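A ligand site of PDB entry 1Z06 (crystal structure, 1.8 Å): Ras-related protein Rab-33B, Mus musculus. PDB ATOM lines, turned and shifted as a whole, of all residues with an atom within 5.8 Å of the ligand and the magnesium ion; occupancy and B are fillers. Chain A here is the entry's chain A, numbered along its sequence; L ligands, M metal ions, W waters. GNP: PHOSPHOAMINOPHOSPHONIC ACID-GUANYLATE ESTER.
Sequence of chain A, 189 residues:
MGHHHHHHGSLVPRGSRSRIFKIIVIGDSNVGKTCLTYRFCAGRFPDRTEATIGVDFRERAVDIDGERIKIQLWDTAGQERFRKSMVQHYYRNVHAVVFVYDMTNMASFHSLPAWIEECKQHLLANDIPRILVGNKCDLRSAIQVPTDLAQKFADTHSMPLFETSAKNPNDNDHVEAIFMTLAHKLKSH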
ATOM      1  N   GLY A  27      23.004  22.116 -27.336  1.00  0.00           N
ATOM      2  CA  GLY A  27      24.352  21.535 -27.364  1.00  0.00           C
ATOM      3  C   GLY A  27      24.991  21.392 -25.997  1.00  0.00           C
ATOM      4  O   GLY A  27      24.453  21.841 -24.995  1.00  0.00           O
ATOM      5  N   ASP A  28      26.152  20.729 -25.969  1.00  0.00           N
ATOM      6  CA  ASP A  28      26.895  20.453 -24.734  1.00  0.00           C
ATOM      7  C   ASP A  28      27.228  21.727 -23.957  1.00  0.00           C
ATOM      8  O   ASP A  28      27.375  22.808 -24.550  1.00  0.00           O
ATOM      9  CB  ASP A  28      28.223  19.739 -25.032  1.00  0.00           C
ATOM     10  CG  ASP A  28      28.071  18.264 -25.380  1.00  0.00           C
ATOM     11  OD1 ASP A  28      26.926  17.755 -25.447  1.00  0.00           O
ATOM     12  OD2 ASP A  28      29.109  17.590 -25.583  1.00  0.00           O
ATOM     13  N   SER A  29      27.358  21.596 -22.642  1.00  0.00           N
ATOM     14  CA  SER A  29      27.857  22.670 -21.810  1.00  0.00           C
ATOM     15  C   SER A  29      29.232  23.106 -22.308  1.00  0.00           C
ATOM     16  O   SER A  29      30.050  22.274 -22.671  1.00  0.00           O
ATOM     17  CB  SER A  29      27.912  22.221 -20.338  1.00  0.00           C
ATOM     18  OG  SER A  29      28.258  23.281 -19.477  1.00  0.00           O
ATOM     19  N   ASN A  30      29.424  24.415 -22.378  1.00  0.00           N
ATOM     20  CA  ASN A  30      30.707  25.095 -22.670  1.00  0.00           C
ATOM     21  C   ASN A  30      31.006  25.318 -24.155  1.00  0.00           C
ATOM     22  O   ASN A  30      32.073  25.809 -24.488  1.00  0.00           O
ATOM     23  CB  ASN A  30      31.913  24.427 -21.975  1.00  0.00           C
ATOM     24  CG  ASN A  30      33.040  25.422 -21.668  1.00  0.00           C
ATOM     25  OD1 ASN A  30      32.819  26.427 -20.993  1.00  0.00           O
ATOM     26  ND2 ASN A  30      34.226  25.157 -22.181  1.00  0.00           N
ATOM     27  N   VAL A  31      30.070  24.977 -25.040  1.00  0.00           N
ATOM     28  CA  VAL A  31      30.292  25.146 -26.471  1.00  0.00           C
ATOM     29  C   VAL A  31      30.144  26.600 -26.926  1.00  0.00           C
ATOM     30  O   VAL A  31      30.618  26.976 -27.990  1.00  0.00           O
ATOM     31  CB  VAL A  31      29.414  24.213 -27.353  1.00  0.00           C
ATOM     32  CG1 VAL A  31      29.625  22.737 -26.976  1.00  0.00           C
ATOM     33  CG2 VAL A  31      27.947  24.609 -27.262  1.00  0.00           C
ATOM     34  N   GLY A  32      29.478  27.414 -26.107  1.00  0.00           N
ATOM     35  CA  GLY A  32      29.329  28.847 -26.393  1.00  0.00           C
ATOM     36  C   GLY A  32      27.923  29.285 -26.760  1.00  0.00           C
ATOM     37  O   GLY A  32      27.754  30.321 -27.417  1.00  0.00           O
ATOM     38  N   LYS A  33      26.893  28.541 -26.340  1.00  0.00           N
ATOM     39  CA  LYS A  33      25.509  28.879 -26.700  1.00  0.00           C
ATOM     40  C   LYS A  33      25.093  30.251 -26.154  1.00  0.00           C
ATOM     41  O   LYS A  33      24.525  31.081 -26.877  1.00  0.00           O
ATOM     42  CB  LYS A  33      24.547  27.789 -26.211  1.00  0.00           C
ATOM     43  CG  LYS A  33      24.891  26.410 -26.764  1.00  0.00           C
ATOM     44  CD  LYS A  33      23.901  25.351 -26.340  1.00  0.00           C
ATOM     45  CE  LYS A  33      23.897  25.115 -24.843  1.00  0.00           C
ATOM     46  NZ  LYS A  33      25.265  24.802 -24.288  1.00  0.00           N
ATOM     47  N   THR A  34      25.403  30.501 -24.882  1.00  0.00           N
ATOM     48  CA  THR A  34      25.122  31.796 -24.244  1.00  0.00           C
ATOM     49  C   THR A  34      25.851  32.942 -24.977  1.00  0.00           C
ATOM     50  O   THR A  34      25.271  33.990 -25.269  1.00  0.00           O
ATOM     51  CB  THR A  34      25.446  31.733 -22.722  1.00  0.00           C
ATOM     52  OG1 THR A  34      24.585  30.772 -22.091  1.00  0.00           O
ATOM     53  CG2 THR A  34      25.277  33.103 -22.028  1.00  0.00           C
ATOM     54  N   CYS A  35      27.113  32.708 -25.321  1.00  0.00           N
ATOM     55  CA  CYS A  35      27.889  33.714 -26.043  1.00  0.00           C
ATOM     56  C   CYS A  35      27.352  34.002 -27.446  1.00  0.00           C
ATOM     57  O   CYS A  35      27.332  35.158 -27.873  1.00  0.00           O
ATOM     58  CB  CYS A  35      29.360  33.317 -26.101  1.00  0.00           C
ATOM     59  SG  CYS A  35      30.169  33.435 -24.495  1.00  0.00           S
ATOM     60  N   LEU A  36      26.907  32.967 -28.155  1.00  0.00           N
ATOM     61  CA  LEU A  36      26.318  33.129 -29.486  1.00  0.00           C
ATOM     62  C   LEU A  36      25.012  33.891 -29.443  1.00  0.00           C
ATOM     63  O   LEU A  36      24.776  34.800 -30.244  1.00  0.00           O
ATOM     64  CB  LEU A  36      26.079  31.772 -30.158  1.00  0.00           C
ATOM     65  CG  LEU A  36      27.325  31.090 -30.703  1.00  0.00           C
ATOM     66  CD1 LEU A  36      27.044  29.609 -30.897  1.00  0.00           C
ATOM     67  CD2 LEU A  36      27.787  31.738 -32.023  1.00  0.00           C
ATOM     68  N   PHE A  45      30.105  40.372 -27.390  1.00  0.00           N
ATOM     69  CA  PHE A  45      30.438  39.151 -26.674  1.00  0.00           C
ATOM     70  C   PHE A  45      30.288  39.375 -25.182  1.00  0.00           C
ATOM     71  O   PHE A  45      30.706  40.417 -24.658  1.00  0.00           O
ATOM     72  CB  PHE A  45      31.880  38.759 -27.023  1.00  0.00           C
ATOM     73  CG  PHE A  45      32.329  37.438 -26.462  1.00  0.00           C
ATOM     74  CD1 PHE A  45      32.031  36.253 -27.114  1.00  0.00           C
ATOM     75  CD2 PHE A  45      33.101  37.389 -25.305  1.00  0.00           C
ATOM     76  CE1 PHE A  45      32.481  35.037 -26.605  1.00  0.00           C
ATOM     77  CE2 PHE A  45      33.547  36.187 -24.801  1.00  0.00           C
ATOM     78  CZ  PHE A  45      33.228  35.003 -25.454  1.00  0.00           C
ATOM     79  N   PRO A  46      29.664  38.406 -24.465  1.00  0.00           N
ATOM     80  CA  PRO A  46      29.569  38.521 -23.028  1.00  0.00           C
ATOM     81  C   PRO A  46      30.804  37.938 -22.356  1.00  0.00           C
ATOM     82  O   PRO A  46      31.076  36.753 -22.479  1.00  0.00           O
ATOM     83  CB  PRO A  46      28.325  37.683 -22.687  1.00  0.00           C
ATOM     84  CG  PRO A  46      28.282  36.653 -23.735  1.00  0.00           C
ATOM     85  CD  PRO A  46      29.006  37.181 -24.957  1.00  0.00           C
ATOM     86  N   THR A  49      30.415  34.845 -18.179  1.00  0.00           N
ATOM     87  CA  THR A  49      29.376  33.830 -18.298  1.00  0.00           C
ATOM     88  C   THR A  49      29.621  32.690 -17.333  1.00  0.00           C
ATOM     89  O   THR A  49      30.765  32.381 -16.981  1.00  0.00           O
ATOM     90  CB  THR A  49      29.294  33.269 -19.720  1.00  0.00           C
ATOM     91  OG1 THR A  49      30.561  32.758 -20.117  1.00  0.00           O
ATOM     92  CG2 THR A  49      28.856  34.348 -20.713  1.00  0.00           C
ATOM     93  N   GLU A  50      28.528  32.065 -16.904  1.00  0.00           N
ATOM     94  CA  GLU A  50      28.583  30.863 -16.095  1.00  0.00           C
ATOM     95  C   GLU A  50      27.623  29.866 -16.704  1.00  0.00           C
ATOM     96  O   GLU A  50      26.825  30.222 -17.572  1.00  0.00           O
ATOM     97  CB  GLU A  50      28.168  31.173 -14.666  1.00  0.00           C
ATOM     98  N   ALA A  51      27.680  28.616 -16.263  1.00  0.00           N
ATOM     99  CA  ALA A  51      26.779  27.589 -16.786  1.00  0.00           C
ATOM    100  C   ALA A  51      25.357  28.064 -16.641  1.00  0.00           C
ATOM    101  O   ALA A  51      24.956  28.569 -15.587  1.00  0.00           O
ATOM    102  CB  ALA A  51      26.968  26.262 -16.069  1.00  0.00           C
ATOM    103  N   THR A  52      24.590  27.928 -17.715  1.00  0.00           N
ATOM    104  CA  THR A  52      23.218  28.424 -17.751  1.00  0.00           C
ATOM    105  C   THR A  52      22.314  27.452 -16.997  1.00  0.00           C
ATOM    106  O   THR A  52      22.427  26.244 -17.152  1.00  0.00           O
ATOM    107  CB  THR A  52      22.743  28.582 -19.190  1.00  0.00           C
ATOM    108  OG1 THR A  52      23.635  29.482 -19.862  1.00  0.00           O
ATOM    109  CG2 THR A  52      21.325  29.108 -19.258  1.00  0.00           C
ATOM    110  N   ILE A  53      21.424  27.996 -16.178  1.00  0.00           N
ATOM    111  CA  ILE A  53      20.570  27.159 -15.348  1.00  0.00           C
ATOM    112  C   ILE A  53      19.138  27.529 -15.613  1.00  0.00           C
ATOM    113  O   ILE A  53      18.760  28.684 -15.456  1.00  0.00           O
ATOM    114  CB  ILE A  53      20.929  27.339 -13.889  1.00  0.00           C
ATOM    115  N   ASP A  75      18.559  30.098 -25.035  1.00  0.00           N
ATOM    116  CA  ASP A  75      19.883  29.750 -24.702  1.00  0.00           C
ATOM    117  C   ASP A  75      19.841  28.553 -23.754  1.00  0.00           C
ATOM    118  O   ASP A  75      19.997  28.720 -22.534  1.00  0.00           O
ATOM    119  CB  ASP A  75      20.461  30.979 -23.985  1.00  0.00           C
ATOM    120  CG  ASP A  75      21.836  30.770 -23.568  1.00  0.00           C
ATOM    121  OD1 ASP A  75      22.250  31.488 -22.629  1.00  0.00           O
ATOM    122  OD2 ASP A  75      22.493  29.897 -24.171  1.00  0.00           O
ATOM    123  N   THR A  76      19.642  27.337 -24.288  1.00  0.00           N
ATOM    124  CA  THR A  76      19.374  26.160 -23.441  1.00  0.00           C
ATOM    125  C   THR A  76      20.554  25.759 -22.561  1.00  0.00           C
ATOM    126  O   THR A  76      21.704  26.089 -22.843  1.00  0.00           O
ATOM    127  CB  THR A  76      18.941  24.921 -24.264  1.00  0.00           C
ATOM    128  OG1 THR A  76      20.033  24.385 -25.014  1.00  0.00           O
ATOM    129  CG2 THR A  76      17.778  25.282 -25.215  1.00  0.00           C
ATOM    130  N   ALA A  77      20.249  25.056 -21.469  1.00  0.00           N
ATOM    131  CA  ALA A  77      21.285  24.563 -20.551  1.00  0.00           C
ATOM    132  C   ALA A  77      21.909  23.294 -21.128  1.00  0.00           C
ATOM    133  O   ALA A  77      21.196  22.392 -21.595  1.00  0.00           O
ATOM    134  CB  ALA A  77      20.693  24.307 -19.156  1.00  0.00           C
ATOM    135  N   GLY A  78      23.235  23.225 -21.107  1.00  0.00           N
ATOM    136  CA  GLY A  78      23.967  22.051 -21.551  1.00  0.00           C
ATOM    137  C   GLY A  78      24.126  21.045 -20.423  1.00  0.00           C
ATOM    138  O   GLY A  78      24.232  19.834 -20.662  1.00  0.00           O
ATOM    139  N   GLN A  79      24.166  21.549 -19.182  1.00  0.00           N
ATOM    140  CA  GLN A  79      24.336  20.672 -18.028  1.00  0.00           C
ATOM    141  C   GLN A  79      23.050  19.932 -17.671  1.00  0.00           C
ATOM    142  O   GLN A  79      21.988  20.510 -17.560  1.00  0.00           O
ATOM    143  CB  GLN A  79      24.868  21.462 -16.840  1.00  0.00           C
ATOM    144  CG  GLN A  79      26.285  21.981 -17.092  1.00  0.00           C
ATOM    145  CD  GLN A  79      27.026  22.385 -15.831  1.00  0.00           C
ATOM    146  OE1 GLN A  79      26.719  21.924 -14.737  1.00  0.00           O
ATOM    147  NE2 GLN A  79      28.004  23.260 -15.979  1.00  0.00           N
ATOM    148  N   ASN A 135      31.434  26.325 -33.208  1.00  0.00           N
ATOM    149  CA  ASN A 135      31.816  27.603 -32.594  1.00  0.00           C
ATOM    150  C   ASN A 135      33.297  27.592 -32.201  1.00  0.00           C
ATOM    151  O   ASN A 135      33.942  26.547 -32.211  1.00  0.00           O
ATOM    152  CB  ASN A 135      30.925  27.865 -31.375  1.00  0.00           C
ATOM    153  CG  ASN A 135      31.064  29.286 -30.834  1.00  0.00           C
ATOM    154  OD1 ASN A 135      31.250  30.249 -31.596  1.00  0.00           O
ATOM    155  ND2 ASN A 135      30.974  29.421 -29.533  1.00  0.00           N
ATOM    156  N   LYS A 136      33.813  28.789 -31.889  1.00  0.00           N
ATOM    157  CA  LYS A 136      35.181  29.000 -31.409  1.00  0.00           C
ATOM    158  C   LYS A 136      36.206  28.804 -32.526  1.00  0.00           C
ATOM    159  O   LYS A 136      37.316  28.343 -32.265  1.00  0.00           O
ATOM    160  CB  LYS A 136      35.519  28.111 -30.199  1.00  0.00           C
ATOM    161  CG  LYS A 136      34.470  28.117 -29.094  1.00  0.00           C
ATOM    162  CD  LYS A 136      35.038  27.647 -27.782  1.00  0.00           C
ATOM    163  CE  LYS A 136      33.936  27.496 -26.743  1.00  0.00           C
ATOM    164  NZ  LYS A 136      34.434  26.869 -25.466  1.00  0.00           N
ATOM    165  N   CYS A 137      35.843  29.179 -33.740  1.00  0.00           N
ATOM    166  CA  CYS A 137      36.751  29.028 -34.905  1.00  0.00           C
ATOM    167  C   CYS A 137      37.941  29.971 -34.814  1.00  0.00           C
ATOM    168  O   CYS A 137      38.913  29.818 -35.561  1.00  0.00           O
ATOM    169  CB  CYS A 137      36.014  29.242 -36.223  1.00  0.00           C
ATOM    170  SG  CYS A 137      35.598  30.934 -36.649  1.00  0.00           S
ATOM    171  N   ASP A 138      37.869  30.935 -33.900  1.00  0.00           N
ATOM    172  CA  ASP A 138      38.989  31.872 -33.656  1.00  0.00           C
ATOM    173  C   ASP A 138      40.199  31.194 -33.012  1.00  0.00           C
ATOM    174  O   ASP A 138      41.332  31.670 -33.146  1.00  0.00           O
ATOM    175  CB  ASP A 138      38.526  33.039 -32.784  1.00  0.00           C
ATOM    176  CG  ASP A 138      37.955  32.589 -31.464  1.00  0.00           C
ATOM    177  OD1 ASP A 138      36.894  31.915 -31.490  1.00  0.00           O
ATOM    178  OD2 ASP A 138      38.535  32.902 -30.413  1.00  0.00           O
ATOM    179  N   LEU A 139      39.958  30.092 -32.312  1.00  0.00           N
ATOM    180  CA  LEU A 139      41.021  29.323 -31.663  1.00  0.00           C
ATOM    181  C   LEU A 139      41.648  28.367 -32.684  1.00  0.00           C
ATOM    182  O   LEU A 139      41.615  27.147 -32.510  1.00  0.00           O
ATOM    183  CB  LEU A 139      40.455  28.570 -30.463  1.00  0.00           C
ATOM    184  CG  LEU A 139      39.729  29.422 -29.421  1.00  0.00           C
ATOM    185  CD1 LEU A 139      39.159  28.551 -28.304  1.00  0.00           C
ATOM    186  CD2 LEU A 139      40.644  30.508 -28.857  1.00  0.00           C
ATOM    187  N   THR A 164      31.835  29.258 -37.098  1.00  0.00           N
ATOM    188  CA  THR A 164      31.833  30.665 -36.700  1.00  0.00           C
ATOM    189  C   THR A 164      32.554  30.899 -35.363  1.00  0.00           C
ATOM    190  O   THR A 164      33.143  29.972 -34.785  1.00  0.00           O
ATOM    191  CB  THR A 164      30.373  31.209 -36.635  1.00  0.00           C
ATOM    192  OG1 THR A 164      30.384  32.637 -36.578  1.00  0.00           O
ATOM    193  CG2 THR A 164      29.617  30.660 -35.425  1.00  0.00           C
ATOM    194  N   SER A 165      32.490  32.127 -34.884  1.00  0.00           N
ATOM    195  CA  SER A 165      33.019  32.484 -33.581  1.00  0.00           C
ATOM    196  C   SER A 165      32.136  33.560 -32.968  1.00  0.00           C
ATOM    197  O   SER A 165      31.912  34.605 -33.564  1.00  0.00           O
ATOM    198  CB  SER A 165      34.472  32.977 -33.684  1.00  0.00           C
ATOM    199  OG  SER A 165      34.882  33.654 -32.504  1.00  0.00           O
ATOM    200  N   ALA A 166      31.632  33.286 -31.761  1.00  0.00           N
ATOM    201  CA  ALA A 166      30.880  34.287 -31.024  1.00  0.00           C
ATOM    202  C   ALA A 166      31.799  35.445 -30.617  1.00  0.00           C
ATOM    203  O   ALA A 166      31.362  36.583 -30.506  1.00  0.00           O
ATOM    204  CB  ALA A 166      30.255  33.652 -29.783  1.00  0.00           C
ATOM    205  N   LYS A 167      33.066  35.137 -30.406  1.00  0.00           N
ATOM    206  CA  LYS A 167      34.029  36.092 -29.867  1.00  0.00           C
ATOM    207  C   LYS A 167      34.681  36.983 -30.929  1.00  0.00           C
ATOM    208  O   LYS A 167      34.808  38.183 -30.710  1.00  0.00           O
ATOM    209  CB  LYS A 167      35.090  35.336 -29.061  1.00  0.00           C
ATOM    210  CG  LYS A 167      35.926  36.220 -28.117  1.00  0.00           C
ATOM    211  CD  LYS A 167      36.707  35.367 -27.131  1.00  0.00           C
ATOM    212  CE  LYS A 167      37.362  36.214 -26.041  1.00  0.00           C
ATOM    213  NZ  LYS A 167      38.030  35.367 -25.002  1.00  0.00           N
ATOM    214  N   ASN A 168      35.054  36.399 -32.069  1.00  0.00           N
ATOM    215  CA  ASN A 168      35.968  37.066 -33.037  1.00  0.00           C
ATOM    216  C   ASN A 168      35.634  37.021 -34.528  1.00  0.00           C
ATOM    217  O   ASN A 168      36.222  37.804 -35.301  1.00  0.00           O
ATOM    218  CB  ASN A 168      37.376  36.509 -32.839  1.00  0.00           C
HETATM  219  PG  GNP L   1      26.126  26.062 -20.701  1.00  0.00           P
HETATM  220  O1G GNP L   1      26.693  25.267 -19.542  1.00  0.00           O
HETATM  221  O2G GNP L   1      25.282  27.227 -20.306  1.00  0.00           O
HETATM  222  O3G GNP L   1      25.442  25.069 -21.605  1.00  0.00           O
HETATM  223  N3B GNP L   1      27.379  26.681 -21.515  1.00  0.00           N
HETATM  224  PB  GNP L   1      27.377  27.522 -22.893  1.00  0.00           P
HETATM  225  O1B GNP L   1      27.313  26.679 -24.110  1.00  0.00           O
HETATM  226  O2B GNP L   1      26.355  28.584 -22.767  1.00  0.00           O
HETATM  227  O3A GNP L   1      28.788  28.214 -22.976  1.00  0.00           O
HETATM  228  PA  GNP L   1      29.176  29.731 -22.797  1.00  0.00           P
HETATM  229  O1A GNP L   1      28.520  30.560 -23.829  1.00  0.00           O
HETATM  230  O2A GNP L   1      29.036  30.106 -21.386  1.00  0.00           O
HETATM  231  O5' GNP L   1      30.707  29.813 -23.171  1.00  0.00           O
HETATM  232  C5' GNP L   1      31.602  28.830 -22.640  1.00  0.00           C
HETATM  233  C4' GNP L   1      33.030  29.330 -22.605  1.00  0.00           C
HETATM  234  O4' GNP L   1      33.554  29.424 -23.947  1.00  0.00           O
HETATM  235  C3' GNP L   1      33.237  30.709 -21.995  1.00  0.00           C
HETATM  236  O3' GNP L   1      34.483  30.758 -21.269  1.00  0.00           O
HETATM  237  C2' GNP L   1      33.253  31.650 -23.187  1.00  0.00           C
HETATM  238  O2' GNP L   1      34.003  32.839 -22.950  1.00  0.00           O
HETATM  239  C1' GNP L   1      33.913  30.763 -24.235  1.00  0.00           C
HETATM  240  N9  GNP L   1      33.526  31.016 -25.605  1.00  0.00           N
HETATM  241  C8  GNP L   1      32.250  30.985 -26.145  1.00  0.00           C
HETATM  242  N7  GNP L   1      32.229  31.236 -27.422  1.00  0.00           N
HETATM  243  C5  GNP L   1      33.563  31.434 -27.763  1.00  0.00           C
HETATM  244  C6  GNP L   1      34.173  31.738 -29.005  1.00  0.00           C
HETATM  245  O6  GNP L   1      33.648  31.900 -30.134  1.00  0.00           O
HETATM  246  N1  GNP L   1      35.551  31.866 -28.911  1.00  0.00           N
HETATM  247  C2  GNP L   1      36.269  31.703 -27.752  1.00  0.00           C
HETATM  248  N2  GNP L   1      37.592  31.875 -27.889  1.00  0.00           N
HETATM  249  N3  GNP L   1      35.725  31.433 -26.567  1.00  0.00           N
HETATM  250  C4  GNP L   1      34.373  31.294 -26.646  1.00  0.00           C
HETATM  251 MG    MG M   1      25.039  28.971 -21.301  1.00  0.00          MG
HETATM  252  O   HOH W   1      30.007  29.358 -18.898  1.00  0.00           O
HETATM  253  O   HOH W   2      36.690  28.141 -24.530  1.00  0.00           O
HETATM  254  O   HOH W   3      32.281  34.569 -21.572  1.00  0.00           O
HETATM  255  O   HOH W   4      30.142  26.838 -19.402  1.00  0.00           O
HETATM  256  O   HOH W   5      36.584  33.461 -23.718  1.00  0.00           O
HETATM  257  O   HOH W   6      24.182  24.440 -18.159  1.00  0.00           O
HETATM  258  O   HOH W   7      35.007  33.126 -19.802  1.00  0.00           O
HETATM  259  O   HOH W   8      26.470  30.024 -20.216  1.00  0.00           O
HETATM  260  O   HOH W   9      23.470  28.111 -22.320  1.00  0.00           O
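O of Val 31 is in hydrogen-bond range of ND2 of Asn 135 (2.9 Å). The backbone NH (N) of Ser 165 lies within hydrogen-bond range of the side-chain sulfur (SG) of Cys 137, 3.8 Å away. The side-chain amino group (NZ) of Lys 136 lies within hydrogen-bond range of the backbone carbonyl oxygen (O) of Asn 30, 2.8 Å away. NZ of Lys 33 lies within hydrogen-bond range of O of Gly 27 (3.2 Å). N of Asn 168 is in hydrogen-bond range of OG of Ser 165, 2.8 Å away. The side-chain carboxylate (OD1) of Asp 138 lies within hydrogen-bond range of the side-chain hydroxyl (OG) of Ser 165. The side-chain amide oxygen of Asn 135 lies within hydrogen-bond range of the backbone NH of Ala 166, 3.1 Å away. The backbone NH (N) of Thr 34 sits at hydrogen-bond distance from the side-chain carboxylate (OD2) of Asp 75, 3.1 Å away.
An oxygen (O6) of the ligand is in hydrogen-bond range of the backbone NH (N) of Ala 166, 2.9 Å away. N of Thr 52 sits close to O2G of the ligand (2.8 Å). N of Lys 167 lies within hydrogen-bond range of O6 of the ligand (3.3 Å). The side-chain amide nitrogen of Asn 135 lies within hydrogen-bond range of a nitrogen (N7) of the ligand (3.1 Å). An oxygen (O3G) of the ligand lies within salt-bridge range of the side-chain amino group (NZ) of Lys 33. An oxygen (O1A) of the ligand sits at hydrogen-bond distance from the backbone NH of Cys 35, 3.0 Å away. N of Gly 32 is in hydrogen-bond range of O1B of the ligand. An oxygen (O3G) of the ligand is in hydrogen-bond range of the backbone NH (N) of Gly 78. The backbone NH (N) of Val 31 is in hydrogen-bond range of an oxygen (O1B) of the ligand (3.4 Å). An oxygen (O1A) of the ligand is in hydrogen-bond range of the backbone NH of Thr 34. The side-chain hydroxyl of Ser 29 lies within hydrogen-bond range of an oxygen (O1G) of the ligand. The side-chain sulfur (SG) of Cys 35 lies within hydrogen-bond range of an oxygen (O1A) of the ligand. N2 of the ligand sits at hydrogen-bond distance from OD2 of Asp 138. N of Lys 33 sits at hydrogen-bond distance from O1B of the ligand. The side-chain hydroxyl (OG1) of Thr 49 sits at hydrogen-bond distance from an oxygen (O2A) of the ligand (3.3 Å). O4' of the ligand sits at hydrogen-bond distance from NZ of Lys 136 (3.1 Å). An oxygen (O6) of the ligand is in hydrogen-bond range of the side-chain hydroxyl (OG) of Ser 165, 3.2 Å away.
Merely in contact with the magnesium ion: Asp 75. Within 4 Å of the magnesium ion: Thr 34, Thr 52 and Asp 75. Along chain A the residues within 4 Å of the magnesium ion span positions 34 to 75.
The backbone NH (N) of Asn 30 lies close to a nitrogen (N3B) of the ligand (3.2 Å). Asp 28 touches the ligand. CZ of Phe 45 touches O2' of the ligand, 3.4 Å away. CA of Ala 51 touches O1G of the ligand, 3.6 Å away. Ala 77 touches the ligand (C to O3G, 3.98 Å). Leu 139 touches the ligand (CD2 to N2, 3.5 Å). Hydrophobic or aromatic side chains within 4 Å of the ligand: Val 31, Phe 45, Ala 51, Leu 139 and Ala 166. The nearest printed residue that does not touch the ligand is Thr 76 (4.1 Å).
O2B of the ligand is bound to the magnesium ion (2.0 Å). The magnesium ion is bound by OG1 of Thr 34. The magnesium ion is bound by an oxygen (O2G) of the ligand (2.0 Å). The magnesium ion is bound by water W9, 2.1 Å away. The magnesium ion is bound by OG1 of Thr 52, 2.1 Å away. Water W8 binds the magnesium ion. The magnesium ion has six donor atoms within binding distance.
Water W9 lies within hydrogen-bond range of the backbone carbonyl oxygen (O) of Thr 76 (2.7 Å) and the side-chain carboxylate (OD2) of Asp 75 (2.8 Å). Water W5 bridges the side-chain amino group of Lys 167 (2.7 Å) and an oxygen (O2') of the ligand (2.8 Å). Water W3 lies within hydrogen-bond range of the backbone carbonyl oxygen (O) of Pro 46, an oxygen (O2') of the ligand, the side-chain hydroxyl (OG1) of Thr 49 and the side-chain sulfur (SG) of Cys 35. Water W6 lies within hydrogen-bond range of the backbone carbonyl oxygen (O) of Thr 52, an oxygen (O1G) of the ligand, the backbone NH (N) of Gln 79 and the backbone NH (N) of Gly 78. Water W2 bridges the side-chain amino group (NZ) of Lys 136 (2.8 Å) and an oxygen (O4') of the ligand (3.4 Å). Water W4 bridges OD1 of Asn 30 and N3B of the ligand.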
